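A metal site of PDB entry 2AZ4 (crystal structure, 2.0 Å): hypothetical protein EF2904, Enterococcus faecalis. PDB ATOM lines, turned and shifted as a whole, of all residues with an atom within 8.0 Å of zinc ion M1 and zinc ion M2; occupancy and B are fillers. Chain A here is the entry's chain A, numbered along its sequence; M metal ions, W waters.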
ATOM      1  N   ILE A  18       5.615 -20.150 -34.414  1.00  0.00           N
ATOM      2  CA  ILE A  18       6.032 -20.625 -33.103  1.00  0.00           C
ATOM      3  C   ILE A  18       6.791 -21.921 -33.300  1.00  0.00           C
ATOM      4  O   ILE A  18       6.210 -23.006 -33.284  1.00  0.00           O
ATOM      5  CB  ILE A  18       4.818 -20.732 -32.151  1.00  0.00           C
ATOM      6  CG1 ILE A  18       4.146 -19.349 -32.072  1.00  0.00           C
ATOM      7  CG2 ILE A  18       5.280 -21.238 -30.783  1.00  0.00           C
ATOM      8  CD1 ILE A  18       3.141 -19.154 -30.948  1.00  0.00           C
ATOM      9  N   GLY A  19       8.086 -21.798 -33.572  1.00  0.00           N
ATOM     10  CA  GLY A  19       8.939 -22.955 -33.784  1.00  0.00           C
ATOM     11  C   GLY A  19       9.992 -22.700 -34.825  1.00  0.00           C
ATOM     12  O   GLY A  19       9.746 -22.019 -35.821  1.00  0.00           O
ATOM     13  N   GLY A  20      11.175 -23.252 -34.596  1.00  0.00           N
ATOM     14  CA  GLY A  20      12.237 -23.181 -35.590  1.00  0.00           C
ATOM     15  C   GLY A  20      13.076 -21.922 -35.519  1.00  0.00           C
ATOM     16  O   GLY A  20      13.706 -21.563 -36.511  1.00  0.00           O
ATOM     17  N   THR A  21      13.107 -21.276 -34.344  1.00  0.00           N
ATOM     18  CA  THR A  21      14.057 -20.184 -34.099  1.00  0.00           C
ATOM     19  C   THR A  21      15.489 -20.629 -34.310  1.00  0.00           C
ATOM     20  O   THR A  21      15.973 -21.560 -33.648  1.00  0.00           O
ATOM     21  CB  THR A  21      13.952 -19.583 -32.688  1.00  0.00           C
ATOM     22  OG1 THR A  21      12.635 -19.086 -32.479  1.00  0.00           O
ATOM     23  CG2 THR A  21      14.896 -18.408 -32.513  1.00  0.00           C
ATOM     24  N   ASP A  35      18.100 -21.699 -31.519  1.00  0.00           N
ATOM     25  CA  ASP A  35      18.252 -23.108 -31.159  1.00  0.00           C
ATOM     26  C   ASP A  35      18.444 -23.901 -32.463  1.00  0.00           C
ATOM     27  O   ASP A  35      19.212 -23.461 -33.332  1.00  0.00           O
ATOM     28  CB  ASP A  35      17.011 -23.569 -30.361  1.00  0.00           C
ATOM     29  CG  ASP A  35      16.944 -22.910 -28.981  1.00  0.00           C
ATOM     30  OD1 ASP A  35      18.006 -22.807 -28.327  1.00  0.00           O
ATOM     31  OD2 ASP A  35      15.839 -22.530 -28.525  1.00  0.00           O
ATOM     32  N   SER A  91      18.254 -24.330 -25.938  1.00  0.00           N
ATOM     33  CA  SER A  91      17.605 -23.784 -24.762  1.00  0.00           C
ATOM     34  C   SER A  91      16.921 -24.884 -23.948  1.00  0.00           C
ATOM     35  O   SER A  91      17.036 -24.902 -22.738  1.00  0.00           O
ATOM     36  CB  SER A  91      16.598 -22.650 -25.128  1.00  0.00           C
ATOM     37  OG  SER A  91      15.370 -23.124 -25.678  1.00  0.00           O
ATOM     38  N   HIS A  92      16.212 -25.775 -24.633  1.00  0.00           N
ATOM     39  CA  HIS A  92      15.498 -26.882 -24.004  1.00  0.00           C
ATOM     40  C   HIS A  92      15.091 -27.955 -25.025  1.00  0.00           C
ATOM     41  O   HIS A  92      15.253 -27.780 -26.245  1.00  0.00           O
ATOM     42  CB  HIS A  92      14.295 -26.393 -23.165  1.00  0.00           C
ATOM     43  CG  HIS A  92      13.202 -25.746 -23.965  1.00  0.00           C
ATOM     44  ND1 HIS A  92      13.414 -24.625 -24.751  1.00  0.00           N
ATOM     45  CD2 HIS A  92      11.891 -26.047 -24.099  1.00  0.00           C
ATOM     46  CE1 HIS A  92      12.263 -24.254 -25.302  1.00  0.00           C
ATOM     47  NE2 HIS A  92      11.333 -25.114 -24.935  1.00  0.00           N
ATOM     48  N   ALA A  93      14.529 -29.058 -24.529  1.00  0.00           N
ATOM     49  CA  ALA A  93      14.256 -30.260 -25.327  1.00  0.00           C
ATOM     50  C   ALA A  93      13.075 -30.214 -26.313  1.00  0.00           C
ATOM     51  O   ALA A  93      13.018 -31.016 -27.272  1.00  0.00           O
ATOM     52  CB  ALA A  93      14.134 -31.468 -24.406  1.00  0.00           C
ATOM     53  N   HIS A  94      12.138 -29.301 -26.084  1.00  0.00           N
ATOM     54  CA  HIS A  94      10.926 -29.259 -26.907  1.00  0.00           C
ATOM     55  C   HIS A  94      11.216 -29.321 -28.389  1.00  0.00           C
ATOM     56  O   HIS A  94      12.215 -28.784 -28.869  1.00  0.00           O
ATOM     57  CB  HIS A  94      10.035 -28.043 -26.523  1.00  0.00           C
ATOM     58  CG  HIS A  94       9.298 -28.249 -25.242  1.00  0.00           C
ATOM     59  ND1 HIS A  94       8.763 -27.201 -24.515  1.00  0.00           N
ATOM     60  CD2 HIS A  94       8.981 -29.368 -24.558  1.00  0.00           C
ATOM     61  CE1 HIS A  94       8.170 -27.674 -23.427  1.00  0.00           C
ATOM     62  NE2 HIS A  94       8.286 -28.988 -23.431  1.00  0.00           N
ATOM     63  N   LEU A  95      10.332 -30.009 -29.116  1.00  0.00           N
ATOM     64  CA  LEU A  95      10.531 -30.314 -30.544  1.00  0.00           C
ATOM     65  C   LEU A  95      10.850 -29.089 -31.430  1.00  0.00           C
ATOM     66  O   LEU A  95      11.709 -29.155 -32.333  1.00  0.00           O
ATOM     67  CB  LEU A  95       9.260 -31.014 -31.065  1.00  0.00           C
ATOM     68  CG  LEU A  95       9.280 -31.704 -32.431  1.00  0.00           C
ATOM     69  CD1 LEU A  95      10.299 -32.867 -32.470  1.00  0.00           C
ATOM     70  CD2 LEU A  95       7.864 -32.185 -32.812  1.00  0.00           C
ATOM     71  N   ASP A  96      10.142 -27.979 -31.137  1.00  0.00           N
ATOM     72  CA  ASP A  96      10.236 -26.740 -31.913  1.00  0.00           C
ATOM     73  C   ASP A  96      11.552 -25.995 -31.669  1.00  0.00           C
ATOM     74  O   ASP A  96      11.829 -24.987 -32.329  1.00  0.00           O
ATOM     75  CB  ASP A  96       9.008 -25.829 -31.676  1.00  0.00           C
ATOM     76  CG  ASP A  96       8.782 -25.469 -30.200  1.00  0.00           C
ATOM     77  OD1 ASP A  96       8.811 -26.387 -29.336  1.00  0.00           O
ATOM     78  OD2 ASP A  96       8.575 -24.260 -29.895  1.00  0.00           O
ATOM     79  N   HIS A  97      12.362 -26.536 -30.753  1.00  0.00           N
ATOM     80  CA  HIS A  97      13.727 -26.084 -30.485  1.00  0.00           C
ATOM     81  C   HIS A  97      14.812 -27.109 -30.813  1.00  0.00           C
ATOM     82  O   HIS A  97      15.968 -26.743 -30.973  1.00  0.00           O
ATOM     83  CB  HIS A  97      13.847 -25.624 -29.020  1.00  0.00           C
ATOM     84  CG  HIS A  97      12.825 -24.593 -28.653  1.00  0.00           C
ATOM     85  ND1 HIS A  97      13.108 -23.235 -28.619  1.00  0.00           N
ATOM     86  CD2 HIS A  97      11.500 -24.698 -28.418  1.00  0.00           C
ATOM     87  CE1 HIS A  97      12.009 -22.567 -28.354  1.00  0.00           C
ATOM     88  NE2 HIS A  97      11.013 -23.424 -28.199  1.00  0.00           N
ATOM     89  N   HIS A 167      10.320 -23.272 -17.003  1.00  0.00           N
ATOM     90  CA  HIS A 167       9.524 -23.644 -18.197  1.00  0.00           C
ATOM     91  C   HIS A 167       8.969 -25.065 -17.916  1.00  0.00           C
ATOM     92  O   HIS A 167       9.414 -25.733 -17.002  1.00  0.00           O
ATOM     93  CB  HIS A 167      10.393 -23.561 -19.471  1.00  0.00           C
ATOM     94  CG  HIS A 167       9.651 -23.799 -20.755  1.00  0.00           C
ATOM     95  ND1 HIS A 167       8.444 -23.196 -21.052  1.00  0.00           N
ATOM     96  CD2 HIS A 167       9.974 -24.536 -21.846  1.00  0.00           C
ATOM     97  CE1 HIS A 167       8.035 -23.598 -22.247  1.00  0.00           C
ATOM     98  NE2 HIS A 167       8.947 -24.399 -22.755  1.00  0.00           N
ATOM     99  N   ASP A 168       7.978 -25.510 -18.677  1.00  0.00           N
ATOM    100  CA  ASP A 168       7.422 -26.841 -18.445  1.00  0.00           C
ATOM    101  C   ASP A 168       8.316 -27.962 -18.998  1.00  0.00           C
ATOM    102  O   ASP A 168       7.966 -29.126 -18.828  1.00  0.00           O
ATOM    103  CB  ASP A 168       5.960 -26.951 -18.940  1.00  0.00           C
ATOM    104  CG  ASP A 168       5.815 -26.682 -20.419  1.00  0.00           C
ATOM    105  OD1 ASP A 168       6.757 -26.127 -20.996  1.00  0.00           O
ATOM    106  OD2 ASP A 168       4.761 -27.024 -21.030  1.00  0.00           O
ATOM    107  N   ALA A 169       9.410 -27.629 -19.692  1.00  0.00           N
ATOM    108  CA  ALA A 169      10.474 -28.600 -19.978  1.00  0.00           C
ATOM    109  C   ALA A 169      11.506 -28.448 -18.882  1.00  0.00           C
ATOM    110  O   ALA A 169      12.051 -27.347 -18.698  1.00  0.00           O
ATOM    111  CB  ALA A 169      11.145 -28.361 -21.339  1.00  0.00           C
ATOM    112  N   ALA A 172      15.329 -26.352 -18.840  1.00  0.00           N
ATOM    113  CA  ALA A 172      15.188 -25.217 -19.753  1.00  0.00           C
ATOM    114  C   ALA A 172      16.116 -24.093 -19.326  1.00  0.00           C
ATOM    115  O   ALA A 172      16.322 -23.874 -18.124  1.00  0.00           O
ATOM    116  CB  ALA A 172      13.748 -24.708 -19.775  1.00  0.00           C
ATOM    117  N   TYR A 186      19.041 -14.139 -24.930  1.00  0.00           N
ATOM    118  CA  TYR A 186      18.046 -14.952 -25.587  1.00  0.00           C
ATOM    119  C   TYR A 186      17.270 -15.668 -24.488  1.00  0.00           C
ATOM    120  O   TYR A 186      17.868 -16.410 -23.721  1.00  0.00           O
ATOM    121  CB  TYR A 186      18.739 -15.973 -26.477  1.00  0.00           C
ATOM    122  CG  TYR A 186      17.806 -17.001 -27.067  1.00  0.00           C
ATOM    123  CD1 TYR A 186      16.680 -16.615 -27.820  1.00  0.00           C
ATOM    124  CD2 TYR A 186      18.007 -18.369 -26.828  1.00  0.00           C
ATOM    125  CE1 TYR A 186      15.818 -17.583 -28.372  1.00  0.00           C
ATOM    126  CE2 TYR A 186      17.151 -19.330 -27.359  1.00  0.00           C
ATOM    127  CZ  TYR A 186      16.060 -18.938 -28.134  1.00  0.00           C
ATOM    128  OH  TYR A 186      15.224 -19.876 -28.664  1.00  0.00           O
ATOM    129  N   GLY A 188      14.932 -17.998 -24.514  1.00  0.00           N
ATOM    130  CA  GLY A 188      14.358 -19.319 -24.759  1.00  0.00           C
ATOM    131  C   GLY A 188      12.869 -19.192 -24.469  1.00  0.00           C
ATOM    132  O   GLY A 188      12.294 -18.094 -24.631  1.00  0.00           O
ATOM    133  N   ASP A 189      12.265 -20.291 -24.051  1.00  0.00           N
ATOM    134  CA  ASP A 189      10.895 -20.284 -23.541  1.00  0.00           C
ATOM    135  C   ASP A 189      10.929 -20.207 -22.031  1.00  0.00           C
ATOM    136  O   ASP A 189      11.797 -20.834 -21.411  1.00  0.00           O
ATOM    137  CB  ASP A 189      10.211 -21.596 -23.928  1.00  0.00           C
ATOM    138  CG  ASP A 189       9.842 -21.672 -25.374  1.00  0.00           C
ATOM    139  OD1 ASP A 189      10.114 -20.735 -26.160  1.00  0.00           O
ATOM    140  OD2 ASP A 189       9.250 -22.694 -25.732  1.00  0.00           O
ATOM    141  N   LEU A 190       9.979 -19.475 -21.430  1.00  0.00           N
ATOM    142  CA  LEU A 190       9.964 -19.241 -19.978  1.00  0.00           C
ATOM    143  C   LEU A 190       8.670 -18.699 -19.389  1.00  0.00           C
ATOM    144  O   LEU A 190       7.808 -18.190 -20.084  1.00  0.00           O
ATOM    145  CB  LEU A 190      11.103 -18.328 -19.513  1.00  0.00           C
ATOM    146  CG  LEU A 190      11.616 -17.035 -20.165  1.00  0.00           C
ATOM    147  CD1 LEU A 190      10.718 -16.291 -21.147  1.00  0.00           C
ATOM    148  CD2 LEU A 190      12.201 -16.114 -19.140  1.00  0.00           C
ATOM    149  N   GLU A 216      10.679 -14.540 -26.308  1.00  0.00           N
ATOM    150  CA  GLU A 216       9.466 -15.198 -26.743  1.00  0.00           C
ATOM    151  C   GLU A 216       8.190 -14.393 -26.462  1.00  0.00           C
ATOM    152  O   GLU A 216       8.152 -13.547 -25.543  1.00  0.00           O
ATOM    153  CB  GLU A 216       9.339 -16.594 -26.091  1.00  0.00           C
ATOM    154  CG  GLU A 216       9.133 -16.529 -24.591  1.00  0.00           C
ATOM    155  CD  GLU A 216       7.943 -17.356 -24.145  1.00  0.00           C
ATOM    156  OE1 GLU A 216       8.159 -18.395 -23.487  1.00  0.00           O
ATOM    157  OE2 GLU A 216       6.783 -16.963 -24.421  1.00  0.00           O
ATOM    158  N   VAL A 218       4.843 -16.172 -26.871  1.00  0.00           N
ATOM    159  CA  VAL A 218       3.899 -17.233 -27.191  1.00  0.00           C
ATOM    160  C   VAL A 218       2.471 -16.909 -26.692  1.00  0.00           C
ATOM    161  O   VAL A 218       1.519 -16.930 -27.483  1.00  0.00           O
ATOM    162  CB  VAL A 218       4.379 -18.610 -26.684  1.00  0.00           C
ATOM    163  CG1 VAL A 218       3.326 -19.674 -26.913  1.00  0.00           C
ATOM    164  CG2 VAL A 218       5.695 -18.981 -27.375  1.00  0.00           C
ATOM    165  N   GLY A 381       3.387 -23.838 -20.112  1.00  0.00           N
ATOM    166  CA  GLY A 381       4.796 -23.604 -19.916  1.00  0.00           C
ATOM    167  C   GLY A 381       5.256 -22.163 -20.172  1.00  0.00           C
ATOM    168  O   GLY A 381       6.397 -21.826 -19.873  1.00  0.00           O
ATOM    169  N   HIS A 382       4.374 -21.320 -20.732  1.00  0.00           N
ATOM    170  CA  HIS A 382       4.747 -19.958 -21.190  1.00  0.00           C
ATOM    171  C   HIS A 382       4.245 -18.853 -20.286  1.00  0.00           C
ATOM    172  O   HIS A 382       3.191 -18.991 -19.649  1.00  0.00           O
ATOM    173  CB  HIS A 382       4.270 -19.716 -22.627  1.00  0.00           C
ATOM    174  CG  HIS A 382       4.932 -20.605 -23.626  1.00  0.00           C
ATOM    175  ND1 HIS A 382       6.192 -20.357 -24.130  1.00  0.00           N
ATOM    176  CD2 HIS A 382       4.522 -21.769 -24.191  1.00  0.00           C
ATOM    177  CE1 HIS A 382       6.524 -21.330 -24.965  1.00  0.00           C
ATOM    178  NE2 HIS A 382       5.527 -22.184 -25.040  1.00  0.00           N
ATOM    179  N   HIS A 404       9.462 -15.866 -31.556  1.00  0.00           N
ATOM    180  CA  HIS A 404       8.639 -16.985 -31.106  1.00  0.00           C
ATOM    181  C   HIS A 404       7.238 -16.453 -30.756  1.00  0.00           C
ATOM    182  O   HIS A 404       6.744 -16.634 -29.633  1.00  0.00           O
ATOM    183  CB  HIS A 404       9.333 -17.656 -29.898  1.00  0.00           C
ATOM    184  CG  HIS A 404       9.115 -19.136 -29.802  1.00  0.00           C
ATOM    185  ND1 HIS A 404       9.285 -19.986 -30.875  1.00  0.00           N
ATOM    186  CD2 HIS A 404       8.793 -19.919 -28.740  1.00  0.00           C
ATOM    187  CE1 HIS A 404       9.058 -21.227 -30.476  1.00  0.00           C
ATOM    188  NE2 HIS A 404       8.762 -21.213 -29.186  1.00  0.00           N
HETATM  189 ZN    ZN M   1       8.895 -23.109 -27.911  1.00  0.00          ZN
HETATM  190 ZN    ZN M   2       9.050 -24.936 -24.910  1.00  0.00          ZN
HETATM  191  O   HOH W   1       6.900 -24.708 -25.307  1.00  0.00           O
HETATM  192  O   HOH W   2       6.591 -23.121 -27.504  1.00  0.00           O
HETATM  193  O   HOH W   3       8.548 -25.287 -27.146  1.00  0.00           O
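A ring nitrogen (ND1) of His 97 is in hydrogen-bond range of the side-chain carboxylate (OD2) of Asp 35, at 2.8 Å. The side-chain carboxylate of Asp 168 sits close to a ring nitrogen (ND1) of His 167, 3.4 Å away. O of Gly 381 is in hydrogen-bond range of ND1 of His 167 (2.7 Å). The backbone NH of Val 218 lies within hydrogen-bond range of the backbone carbonyl oxygen of His 404 (3.4 Å). A ring nitrogen (ND1) of His 404 sits close to the backbone NH (N) of Gly 19 (3.5 Å). OG of Ser 91 sits at hydrogen-bond distance from ND1 of His 92, 2.6 Å away. O of Asp 96 sits at hydrogen-bond distance from N of Gly 20, at 2.9 Å.
Within 4 Å of zinc ion M1: Asp 96, His 97, Asp 189 and His 404.
Four residues have an atom within 4 Å of zinc ion M2: His 92, His 94, His 167 and Asp 189. The nearest printed residue that does not touch zinc ion M2 is His 97 (4.1 Å).
Zinc ion M1 is bound by a ring nitrogen (NE2) of His 97 (2.2 Å), the side-chain carboxylate of Asp 189 (2.2 Å), a ring nitrogen (NE2) of His 404 (2.3 Å), the side-chain carboxylate of Asp 96 (2.3 Å), water W3 (2.3 Å) and water W2 (2.3 Å).
Zinc ion M2 is bound by water W1, 2.2 Å away. Zinc ion M2 is bound by NE2 of His 167. Zinc ion M2 is bound by NE2 of His 92, 2.3 Å away. Zinc ion M2 is bound by ND1 of His 94 (2.3 Å). Water W3 binds zinc ion M2 (2.3 Å). Zinc ion M2 is bound by OD2 of Asp 189, 2.4 Å away.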
